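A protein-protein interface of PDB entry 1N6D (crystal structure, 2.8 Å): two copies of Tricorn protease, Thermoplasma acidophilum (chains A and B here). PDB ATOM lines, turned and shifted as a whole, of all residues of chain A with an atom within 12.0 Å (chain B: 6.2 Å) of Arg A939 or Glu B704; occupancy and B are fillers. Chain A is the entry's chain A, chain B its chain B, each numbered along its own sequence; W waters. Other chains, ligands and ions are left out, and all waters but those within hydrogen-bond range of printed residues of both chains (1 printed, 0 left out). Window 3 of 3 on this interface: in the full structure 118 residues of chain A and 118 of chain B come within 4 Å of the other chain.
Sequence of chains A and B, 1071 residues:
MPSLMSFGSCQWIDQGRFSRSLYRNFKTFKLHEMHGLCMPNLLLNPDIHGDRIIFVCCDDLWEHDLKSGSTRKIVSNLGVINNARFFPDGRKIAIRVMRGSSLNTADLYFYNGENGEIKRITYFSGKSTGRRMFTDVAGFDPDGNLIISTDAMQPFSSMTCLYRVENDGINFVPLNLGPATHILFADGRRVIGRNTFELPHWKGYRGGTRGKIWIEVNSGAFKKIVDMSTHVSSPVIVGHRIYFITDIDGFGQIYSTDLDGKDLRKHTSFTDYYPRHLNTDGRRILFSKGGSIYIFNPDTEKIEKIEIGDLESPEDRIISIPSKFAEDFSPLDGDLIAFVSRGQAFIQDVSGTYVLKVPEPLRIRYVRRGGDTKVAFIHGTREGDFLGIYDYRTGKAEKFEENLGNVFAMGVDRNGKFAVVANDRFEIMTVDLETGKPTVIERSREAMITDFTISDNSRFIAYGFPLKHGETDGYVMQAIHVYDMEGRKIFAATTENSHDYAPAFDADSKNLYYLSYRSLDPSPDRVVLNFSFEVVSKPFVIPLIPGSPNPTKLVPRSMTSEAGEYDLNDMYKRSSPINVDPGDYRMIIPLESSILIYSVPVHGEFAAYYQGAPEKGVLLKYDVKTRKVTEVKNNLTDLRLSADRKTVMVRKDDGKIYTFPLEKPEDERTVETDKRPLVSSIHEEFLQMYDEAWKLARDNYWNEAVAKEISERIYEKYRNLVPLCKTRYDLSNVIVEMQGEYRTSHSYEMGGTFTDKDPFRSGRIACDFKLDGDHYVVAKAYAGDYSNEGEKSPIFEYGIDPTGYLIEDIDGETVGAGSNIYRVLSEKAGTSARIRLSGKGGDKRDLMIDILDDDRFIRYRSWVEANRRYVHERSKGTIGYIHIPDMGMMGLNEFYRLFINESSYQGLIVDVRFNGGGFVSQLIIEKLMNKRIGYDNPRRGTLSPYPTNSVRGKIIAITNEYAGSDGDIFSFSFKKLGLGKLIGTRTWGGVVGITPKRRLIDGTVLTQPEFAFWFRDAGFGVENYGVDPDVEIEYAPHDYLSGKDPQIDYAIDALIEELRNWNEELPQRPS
No position is printed for both chains.
The side-chain carboxylate (OD2) of Asp A936 sits close to the backbone carbonyl oxygen (O) of Phe B1011 (3.4 Å).
The guanidinium group (NH2) of Arg A939 lies within hydrogen-bond range of the backbone carbonyl oxygen (O) of Tyr B701 (2.5 Å).
O of Glu B1010 lies within hydrogen-bond range of N of Arg A939 (3.2 Å).
O of Glu B1010 lies close to O of Asn A937.
The guanidinium group (NH2) of Arg A939 sits at hydrogen-bond distance from the backbone carbonyl oxygen (O) of Arg B698 (2.9 Å).
The guanidinium group of Arg A939 lies within hydrogen-bond range of the backbone carbonyl oxygen of Asp B699 (3.3 Å).
O of Asp B699 sits at hydrogen-bond distance from NH2 of Arg A940 (3.2 Å).
Hydrophobic or aromatic side chains of chain A that line the printed part of chain B: Pro A938.
Among the printed residues, no Asp or Glu carboxylate lies within 4 Å of a Lys or Arg side-chain nitrogen of the other chain.
O of Ser A944 is in hydrogen-bond range of N of Asp A936, 3.0 Å away.
OD2 of Asp B699 lies within salt-bridge range of NH1 of Arg B698, 3.0 Å away.
OH of Tyr B701 lies within hydrogen-bond range of NE1 of Trp B702 (2.9 Å).
Asn A937 touches Trp B702 (O to CB, 3.97 Å).
O of Asn A937 touches CA of Phe B1011, 3.3 Å away.
Pro A938 touches Glu B1010.
CB of Pro A938 touches CD2 of Phe B1011 (3.8 Å).
CB of Arg A939 touches O of Asn B700 (3.8 Å).
O of Trp B702 touches CA of Arg A939, 3.4 Å away.
Arg A939 touches Glu B704 (NH1 to CG, 3.1 Å).
Arg A939 touches Ala B707.
Arg A940 touches Asn B700 (NH2 to OD1, 3.6 Å).
Water W1 lies within hydrogen-bond range of the side-chain carboxylate of Glu B1010 (2.8 Å) and the guanidinium group of Arg A940 (3.0 Å).
Printed residues of chain B within 4 Å of Pro A938: Glu B1010 and Phe B1011.
Of chain A, only Arg A939 (2.9 Å) comes within 4 Å of Arg B698.
Asp B699 touches just these residues of chain A: Arg A939 and Arg A940.
Asn B700 touches just these residues of chain A: Arg A939 (3.8 Å) and Arg A940 (3.6 Å).
Of the printed residues of chain A, Tyr B701 touches Arg A939 (2.5 Å).
Of chain A, only Asn A937 and Arg A939 come within 4 Å of Trp B702.
Glu B704 touches one residue of chain A.
No residue of chain A comes within 4 Å of Ala B705.
Glu B1010 touches just these residues of chain A: Asn A937 (3.5 Å), Pro A938 (3.4 Å) and Arg A939 (3.2 Å).
Of chain A, only Asp A936 (3.4 Å), Asn A937 (3.3 Å) and Pro A938 (3.8 Å) come within 4 Å of Phe B1011.
The nearest residue of chain B that does not touch Arg A939 is Asn B703 (4.4 Å).
The nearest printed residue of chain B that does not touch Arg A940 is Glu B1010 (4.1 Å).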
ATOM      1  N   TYR A 935      12.995  -1.212  -6.033  1.00  0.00           N
ATOM      2  CA  TYR A 935      11.845  -1.467  -6.874  1.00  0.00           C
ATOM      3  C   TYR A 935      12.249  -1.704  -8.299  1.00  0.00           C
ATOM      4  O   TYR A 935      13.361  -1.390  -8.691  1.00  0.00           O
ATOM      5  CB  TYR A 935      10.854  -0.304  -6.809  1.00  0.00           C
ATOM      6  CG  TYR A 935      10.109  -0.221  -5.510  1.00  0.00           C
ATOM      7  CD1 TYR A 935      10.464   0.723  -4.546  1.00  0.00           C
ATOM      8  CD2 TYR A 935       9.053  -1.097  -5.230  1.00  0.00           C
ATOM      9  CE1 TYR A 935       9.781   0.801  -3.319  1.00  0.00           C
ATOM     10  CE2 TYR A 935       8.365  -1.030  -4.003  1.00  0.00           C
ATOM     11  CZ  TYR A 935       8.736  -0.076  -3.055  1.00  0.00           C
ATOM     12  OH  TYR A 935       8.067  -0.008  -1.850  1.00  0.00           O
ATOM     13  N   ASP A 936      11.326  -2.263  -9.065  1.00  0.00           N
ATOM     14  CA  ASP A 936      11.553  -2.541 -10.473  1.00  0.00           C
ATOM     15  C   ASP A 936      10.533  -1.680 -11.225  1.00  0.00           C
ATOM     16  O   ASP A 936       9.332  -1.804 -10.996  1.00  0.00           O
ATOM     17  CB  ASP A 936      11.287  -4.021 -10.756  1.00  0.00           C
ATOM     18  CG  ASP A 936      12.482  -4.737 -11.336  1.00  0.00           C
ATOM     19  OD1 ASP A 936      12.408  -5.983 -11.448  1.00  0.00           O
ATOM     20  OD2 ASP A 936      13.476  -4.058 -11.684  1.00  0.00           O
ATOM     21  N   ASN A 937      11.006  -0.805 -12.102  1.00  0.00           N
ATOM     22  CA  ASN A 937      10.108   0.039 -12.857  1.00  0.00           C
ATOM     23  C   ASN A 937       9.892  -0.505 -14.235  1.00  0.00           C
ATOM     24  O   ASN A 937      10.811  -0.552 -15.064  1.00  0.00           O
ATOM     25  CB  ASN A 937      10.653   1.441 -12.969  1.00  0.00           C
ATOM     26  CG  ASN A 937      10.827   2.073 -11.641  1.00  0.00           C
ATOM     27  OD1 ASN A 937      11.595   1.588 -10.801  1.00  0.00           O
ATOM     28  ND2 ASN A 937      10.103   3.155 -11.415  1.00  0.00           N
ATOM     29  N   PRO A 938       8.656  -0.933 -14.501  1.00  0.00           N
ATOM     30  CA  PRO A 938       8.303  -1.485 -15.801  1.00  0.00           C
ATOM     31  C   PRO A 938       7.755  -0.453 -16.766  1.00  0.00           C
ATOM     32  O   PRO A 938       7.256   0.599 -16.360  1.00  0.00           O
ATOM     33  CB  PRO A 938       7.249  -2.520 -15.442  1.00  0.00           C
ATOM     34  CG  PRO A 938       6.487  -1.812 -14.380  1.00  0.00           C
ATOM     35  CD  PRO A 938       7.572  -1.181 -13.530  1.00  0.00           C
ATOM     36  N   ARG A 939       7.845  -0.780 -18.046  1.00  0.00           N
ATOM     37  CA  ARG A 939       7.319   0.088 -19.068  1.00  0.00           C
ATOM     38  C   ARG A 939       5.790   0.093 -18.945  1.00  0.00           C
ATOM     39  O   ARG A 939       5.128   1.107 -19.179  1.00  0.00           O
ATOM     40  CB  ARG A 939       7.747  -0.402 -20.448  1.00  0.00           C
ATOM     41  CG  ARG A 939       7.034   0.278 -21.590  1.00  0.00           C
ATOM     42  CD  ARG A 939       7.133   1.782 -21.512  1.00  0.00           C
ATOM     43  NE  ARG A 939       6.648   2.387 -22.738  1.00  0.00           N
ATOM     44  CZ  ARG A 939       7.327   2.412 -23.882  1.00  0.00           C
ATOM     45  NH1 ARG A 939       6.786   2.983 -24.951  1.00  0.00           N
ATOM     46  NH2 ARG A 939       8.541   1.879 -23.962  1.00  0.00           N
ATOM     47  N   ARG A 940       5.236  -1.056 -18.581  1.00  0.00           N
ATOM     48  CA  ARG A 940       3.794  -1.216 -18.392  1.00  0.00           C
ATOM     49  C   ARG A 940       3.536  -2.081 -17.164  1.00  0.00           C
ATOM     50  O   ARG A 940       4.135  -3.140 -17.007  1.00  0.00           O
ATOM     51  CB  ARG A 940       3.142  -1.854 -19.624  1.00  0.00           C
ATOM     52  CG  ARG A 940       3.840  -3.082 -20.179  1.00  0.00           C
ATOM     53  CD  ARG A 940       3.154  -3.511 -21.467  1.00  0.00           C
ATOM     54  NE  ARG A 940       3.073  -2.404 -22.424  1.00  0.00           N
ATOM     55  CZ  ARG A 940       4.079  -2.002 -23.200  1.00  0.00           C
ATOM     56  NH1 ARG A 940       3.920  -0.984 -24.036  1.00  0.00           N
ATOM     57  NH2 ARG A 940       5.245  -2.629 -23.152  1.00  0.00           N
ATOM     58  N   GLY A 941       2.659  -1.618 -16.285  1.00  0.00           N
ATOM     59  CA  GLY A 941       2.381  -2.378 -15.088  1.00  0.00           C
ATOM     60  C   GLY A 941       2.753  -1.585 -13.862  1.00  0.00           C
ATOM     61  O   GLY A 941       3.044  -0.395 -13.949  1.00  0.00           O
ATOM     62  N   THR A 942       2.763  -2.254 -12.718  1.00  0.00           N
ATOM     63  CA  THR A 942       3.069  -1.605 -11.450  1.00  0.00           C
ATOM     64  C   THR A 942       4.478  -1.952 -10.927  1.00  0.00           C
ATOM     65  O   THR A 942       5.162  -2.816 -11.475  1.00  0.00           O
ATOM     66  CB  THR A 942       1.991  -1.989 -10.446  1.00  0.00           C
ATOM     67  OG1 THR A 942       2.037  -3.397 -10.197  1.00  0.00           O
ATOM     68  CG2 THR A 942       0.619  -1.683 -11.038  1.00  0.00           C
ATOM     69  N   LEU A 943       4.913  -1.264  -9.879  1.00  0.00           N
ATOM     70  CA  LEU A 943       6.228  -1.500  -9.320  1.00  0.00           C
ATOM     71  C   LEU A 943       6.367  -2.917  -8.780  1.00  0.00           C
ATOM     72  O   LEU A 943       5.386  -3.534  -8.398  1.00  0.00           O
ATOM     73  CB  LEU A 943       6.502  -0.524  -8.175  1.00  0.00           C
ATOM     74  CG  LEU A 943       6.594   0.953  -8.542  1.00  0.00           C
ATOM     75  CD1 LEU A 943       6.773   1.749  -7.264  1.00  0.00           C
ATOM     76  CD2 LEU A 943       7.771   1.202  -9.508  1.00  0.00           C
ATOM     77  N   SER A 944       7.586  -3.440  -8.767  1.00  0.00           N
ATOM     78  CA  SER A 944       7.823  -4.754  -8.199  1.00  0.00           C
ATOM     79  C   SER A 944       8.778  -4.569  -7.030  1.00  0.00           C
ATOM     80  O   SER A 944       9.928  -4.209  -7.206  1.00  0.00           O
ATOM     81  CB  SER A 944       8.429  -5.685  -9.223  1.00  0.00           C
ATOM     82  OG  SER A 944       7.537  -5.924 -10.260  1.00  0.00           O
ATOM     83  N   ALA B 697      11.912  -2.679 -29.639  1.00  0.00           N
ATOM     84  CA  ALA B 697      12.863  -1.881 -28.900  1.00  0.00           C
ATOM     85  C   ALA B 697      12.182  -0.617 -28.371  1.00  0.00           C
ATOM     86  O   ALA B 697      12.432  -0.177 -27.243  1.00  0.00           O
ATOM     87  CB  ALA B 697      14.047  -1.516 -29.779  1.00  0.00           C
ATOM     88  N   ARG B 698      11.310  -0.028 -29.183  1.00  0.00           N
ATOM     89  CA  ARG B 698      10.611   1.192 -28.778  1.00  0.00           C
ATOM     90  C   ARG B 698       9.471   0.924 -27.817  1.00  0.00           C
ATOM     91  O   ARG B 698       9.327   1.589 -26.772  1.00  0.00           O
ATOM     92  CB  ARG B 698      10.027   1.922 -29.981  1.00  0.00           C
ATOM     93  CG  ARG B 698       9.492   3.297 -29.616  1.00  0.00           C
ATOM     94  CD  ARG B 698       8.555   3.765 -30.692  1.00  0.00           C
ATOM     95  NE  ARG B 698       7.507   2.767 -30.897  1.00  0.00           N
ATOM     96  CZ  ARG B 698       6.679   2.759 -31.931  1.00  0.00           C
ATOM     97  NH1 ARG B 698       5.752   1.811 -32.049  1.00  0.00           N
ATOM     98  NH2 ARG B 698       6.795   3.698 -32.856  1.00  0.00           N
ATOM     99  N   ASP B 699       8.644  -0.047 -28.184  1.00  0.00           N
ATOM    100  CA  ASP B 699       7.493  -0.407 -27.370  1.00  0.00           C
ATOM    101  C   ASP B 699       7.810  -1.008 -25.992  1.00  0.00           C
ATOM    102  O   ASP B 699       7.020  -0.853 -25.068  1.00  0.00           O
ATOM    103  CB  ASP B 699       6.578  -1.326 -28.185  1.00  0.00           C
ATOM    104  CG  ASP B 699       5.868  -0.585 -29.291  1.00  0.00           C
ATOM    105  OD1 ASP B 699       5.311  -1.265 -30.187  1.00  0.00           O
ATOM    106  OD2 ASP B 699       5.874   0.674 -29.243  1.00  0.00           O
ATOM    107  N   ASN B 700       8.973  -1.630 -25.835  1.00  0.00           N
ATOM    108  CA  ASN B 700       9.305  -2.228 -24.559  1.00  0.00           C
ATOM    109  C   ASN B 700      10.318  -1.486 -23.684  1.00  0.00           C
ATOM    110  O   ASN B 700      10.548  -1.871 -22.540  1.00  0.00           O
ATOM    111  CB  ASN B 700       9.768  -3.676 -24.764  1.00  0.00           C
ATOM    112  CG  ASN B 700       8.735  -4.523 -25.487  1.00  0.00           C
ATOM    113  OD1 ASN B 700       7.538  -4.285 -25.369  1.00  0.00           O
ATOM    114  ND2 ASN B 700       9.198  -5.530 -26.227  1.00  0.00           N
ATOM    115  N   TYR B 701      10.944  -0.438 -24.202  1.00  0.00           N
ATOM    116  CA  TYR B 701      11.909   0.295 -23.381  1.00  0.00           C
ATOM    117  C   TYR B 701      11.204   0.713 -22.091  1.00  0.00           C
ATOM    118  O   TYR B 701      10.063   1.175 -22.122  1.00  0.00           O
ATOM    119  CB  TYR B 701      12.443   1.533 -24.117  1.00  0.00           C
ATOM    120  CG  TYR B 701      13.658   2.124 -23.431  1.00  0.00           C
ATOM    121  CD1 TYR B 701      14.796   1.339 -23.220  1.00  0.00           C
ATOM    122  CD2 TYR B 701      13.643   3.426 -22.901  1.00  0.00           C
ATOM    123  CE1 TYR B 701      15.875   1.816 -22.499  1.00  0.00           C
ATOM    124  CE2 TYR B 701      14.729   3.909 -22.169  1.00  0.00           C
ATOM    125  CZ  TYR B 701      15.834   3.086 -21.977  1.00  0.00           C
ATOM    126  OH  TYR B 701      16.891   3.534 -21.235  1.00  0.00           O
ATOM    127  N   TRP B 702      11.890   0.570 -20.962  1.00  0.00           N
ATOM    128  CA  TRP B 702      11.291   0.885 -19.662  1.00  0.00           C
ATOM    129  C   TRP B 702      10.719   2.296 -19.569  1.00  0.00           C
ATOM    130  O   TRP B 702       9.681   2.520 -18.940  1.00  0.00           O
ATOM    131  CB  TRP B 702      12.305   0.680 -18.533  1.00  0.00           C
ATOM    132  CG  TRP B 702      13.327   1.741 -18.471  1.00  0.00           C
ATOM    133  CD1 TRP B 702      14.387   1.919 -19.313  1.00  0.00           C
ATOM    134  CD2 TRP B 702      13.354   2.835 -17.550  1.00  0.00           C
ATOM    135  NE1 TRP B 702      15.068   3.062 -18.972  1.00  0.00           N
ATOM    136  CE2 TRP B 702      14.456   3.641 -17.894  1.00  0.00           C
ATOM    137  CE3 TRP B 702      12.547   3.212 -16.465  1.00  0.00           C
ATOM    138  CZ2 TRP B 702      14.778   4.799 -17.200  1.00  0.00           C
ATOM    139  CZ3 TRP B 702      12.864   4.365 -15.769  1.00  0.00           C
ATOM    140  CH2 TRP B 702      13.976   5.149 -16.141  1.00  0.00           C
ATOM    141  N   ASN B 703      11.393   3.252 -20.199  1.00  0.00           N
ATOM    142  CA  ASN B 703      10.927   4.620 -20.148  1.00  0.00           C
ATOM    143  C   ASN B 703      10.306   5.020 -21.468  1.00  0.00           C
ATOM    144  O   ASN B 703      10.997   5.187 -22.477  1.00  0.00           O
ATOM    145  CB  ASN B 703      12.074   5.562 -19.780  1.00  0.00           C
ATOM    146  CG  ASN B 703      11.651   7.016 -19.778  1.00  0.00           C
ATOM    147  OD1 ASN B 703      12.463   7.898 -19.547  1.00  0.00           O
ATOM    148  ND2 ASN B 703      10.375   7.273 -20.041  1.00  0.00           N
ATOM    149  N   GLU B 704       8.988   5.183 -21.451  1.00  0.00           N
ATOM    150  CA  GLU B 704       8.262   5.545 -22.655  1.00  0.00           C
ATOM    151  C   GLU B 704       8.754   6.837 -23.294  1.00  0.00           C
ATOM    152  O   GLU B 704       8.877   6.928 -24.510  1.00  0.00           O
ATOM    153  CB  GLU B 704       6.783   5.670 -22.343  1.00  0.00           C
ATOM    154  CG  GLU B 704       5.927   5.601 -23.572  1.00  0.00           C
ATOM    155  CD  GLU B 704       4.496   5.961 -23.271  1.00  0.00           C
ATOM    156  OE1 GLU B 704       3.654   5.817 -24.183  1.00  0.00           O
ATOM    157  OE2 GLU B 704       4.217   6.398 -22.128  1.00  0.00           O
ATOM    158  N   ALA B 705       9.020   7.843 -22.470  1.00  0.00           N
ATOM    159  CA  ALA B 705       9.505   9.124 -22.973  1.00  0.00           C
ATOM    160  C   ALA B 705      10.774   8.980 -23.823  1.00  0.00           C
ATOM    161  O   ALA B 705      10.791   9.340 -25.009  1.00  0.00           O
ATOM    162  CB  ALA B 705       9.772  10.070 -21.816  1.00  0.00           C
ATOM    163  N   VAL B 706      11.833   8.465 -23.203  1.00  0.00           N
ATOM    164  CA  VAL B 706      13.118   8.255 -23.862  1.00  0.00           C
ATOM    165  C   VAL B 706      12.941   7.442 -25.129  1.00  0.00           C
ATOM    166  O   VAL B 706      13.666   7.617 -26.104  1.00  0.00           O
ATOM    167  CB  VAL B 706      14.090   7.522 -22.920  1.00  0.00           C
ATOM    168  CG1 VAL B 706      15.393   7.202 -23.635  1.00  0.00           C
ATOM    169  CG2 VAL B 706      14.357   8.382 -21.710  1.00  0.00           C
ATOM    170  N   ALA B 707      11.957   6.555 -25.103  1.00  0.00           N
ATOM    171  CA  ALA B 707      11.651   5.700 -26.240  1.00  0.00           C
ATOM    172  C   ALA B 707      11.169   6.504 -27.463  1.00  0.00           C
ATOM    173  O   ALA B 707      11.694   6.337 -28.574  1.00  0.00           O
ATOM    174  CB  ALA B 707      10.596   4.674 -25.837  1.00  0.00           C
ATOM    175  N   LYS B 708      10.183   7.375 -27.258  1.00  0.00           N
ATOM    176  CA  LYS B 708       9.638   8.180 -28.342  1.00  0.00           C
ATOM    177  C   LYS B 708      10.742   8.951 -29.050  1.00  0.00           C
ATOM    178  O   LYS B 708      10.722   9.093 -30.275  1.00  0.00           O
ATOM    179  N   GLU B 709      11.725   9.424 -28.286  1.00  0.00           N
ATOM    180  CA  GLU B 709      12.834  10.202 -28.859  1.00  0.00           C
ATOM    181  C   GLU B 709      13.906   9.367 -29.546  1.00  0.00           C
ATOM    182  O   GLU B 709      14.244   9.647 -30.674  1.00  0.00           O
ATOM    183  CB  GLU B 709      13.488  11.062 -27.765  1.00  0.00           C
ATOM    184  CG  GLU B 709      14.318  12.261 -28.249  1.00  0.00           C
ATOM    185  CD  GLU B 709      15.722  11.892 -28.655  1.00  0.00           C
ATOM    186  OE1 GLU B 709      16.436  11.243 -27.854  1.00  0.00           O
ATOM    187  OE2 GLU B 709      16.125  12.260 -29.783  1.00  0.00           O
ATOM    188  N   GLU B1010      13.356  -3.448 -20.254  1.00  0.00           N
ATOM    189  CA  GLU B1010      11.983  -3.106 -19.896  1.00  0.00           C
ATOM    190  C   GLU B1010      11.700  -2.897 -18.410  1.00  0.00           C
ATOM    191  O   GLU B1010      10.660  -2.340 -18.047  1.00  0.00           O
ATOM    192  CB  GLU B1010      11.087  -4.216 -20.426  1.00  0.00           C
ATOM    193  CG  GLU B1010       9.612  -3.953 -20.403  1.00  0.00           C
ATOM    194  CD  GLU B1010       8.853  -5.038 -21.138  1.00  0.00           C
ATOM    195  OE1 GLU B1010       9.491  -5.766 -21.929  1.00  0.00           O
ATOM    196  OE2 GLU B1010       7.626  -5.168 -20.938  1.00  0.00           O
ATOM    197  N   PHE B1011      12.621  -3.330 -17.553  1.00  0.00           N
ATOM    198  CA  PHE B1011      12.412  -3.202 -16.119  1.00  0.00           C
ATOM    199  C   PHE B1011      13.550  -2.537 -15.360  1.00  0.00           C
ATOM    200  O   PHE B1011      14.453  -3.202 -14.858  1.00  0.00           O
ATOM    201  CB  PHE B1011      12.123  -4.585 -15.524  1.00  0.00           C
ATOM    202  CG  PHE B1011      11.067  -5.353 -16.267  1.00  0.00           C
ATOM    203  CD1 PHE B1011      11.381  -6.058 -17.417  1.00  0.00           C
ATOM    204  CD2 PHE B1011       9.741  -5.296 -15.863  1.00  0.00           C
ATOM    205  CE1 PHE B1011      10.377  -6.678 -18.150  1.00  0.00           C
ATOM    206  CE2 PHE B1011       8.736  -5.911 -16.586  1.00  0.00           C
ATOM    207  CZ  PHE B1011       9.049  -6.593 -17.717  1.00  0.00           C
HETATM  208  O   HOH W   1       5.334  -5.499 -22.449  1.00  0.00           O
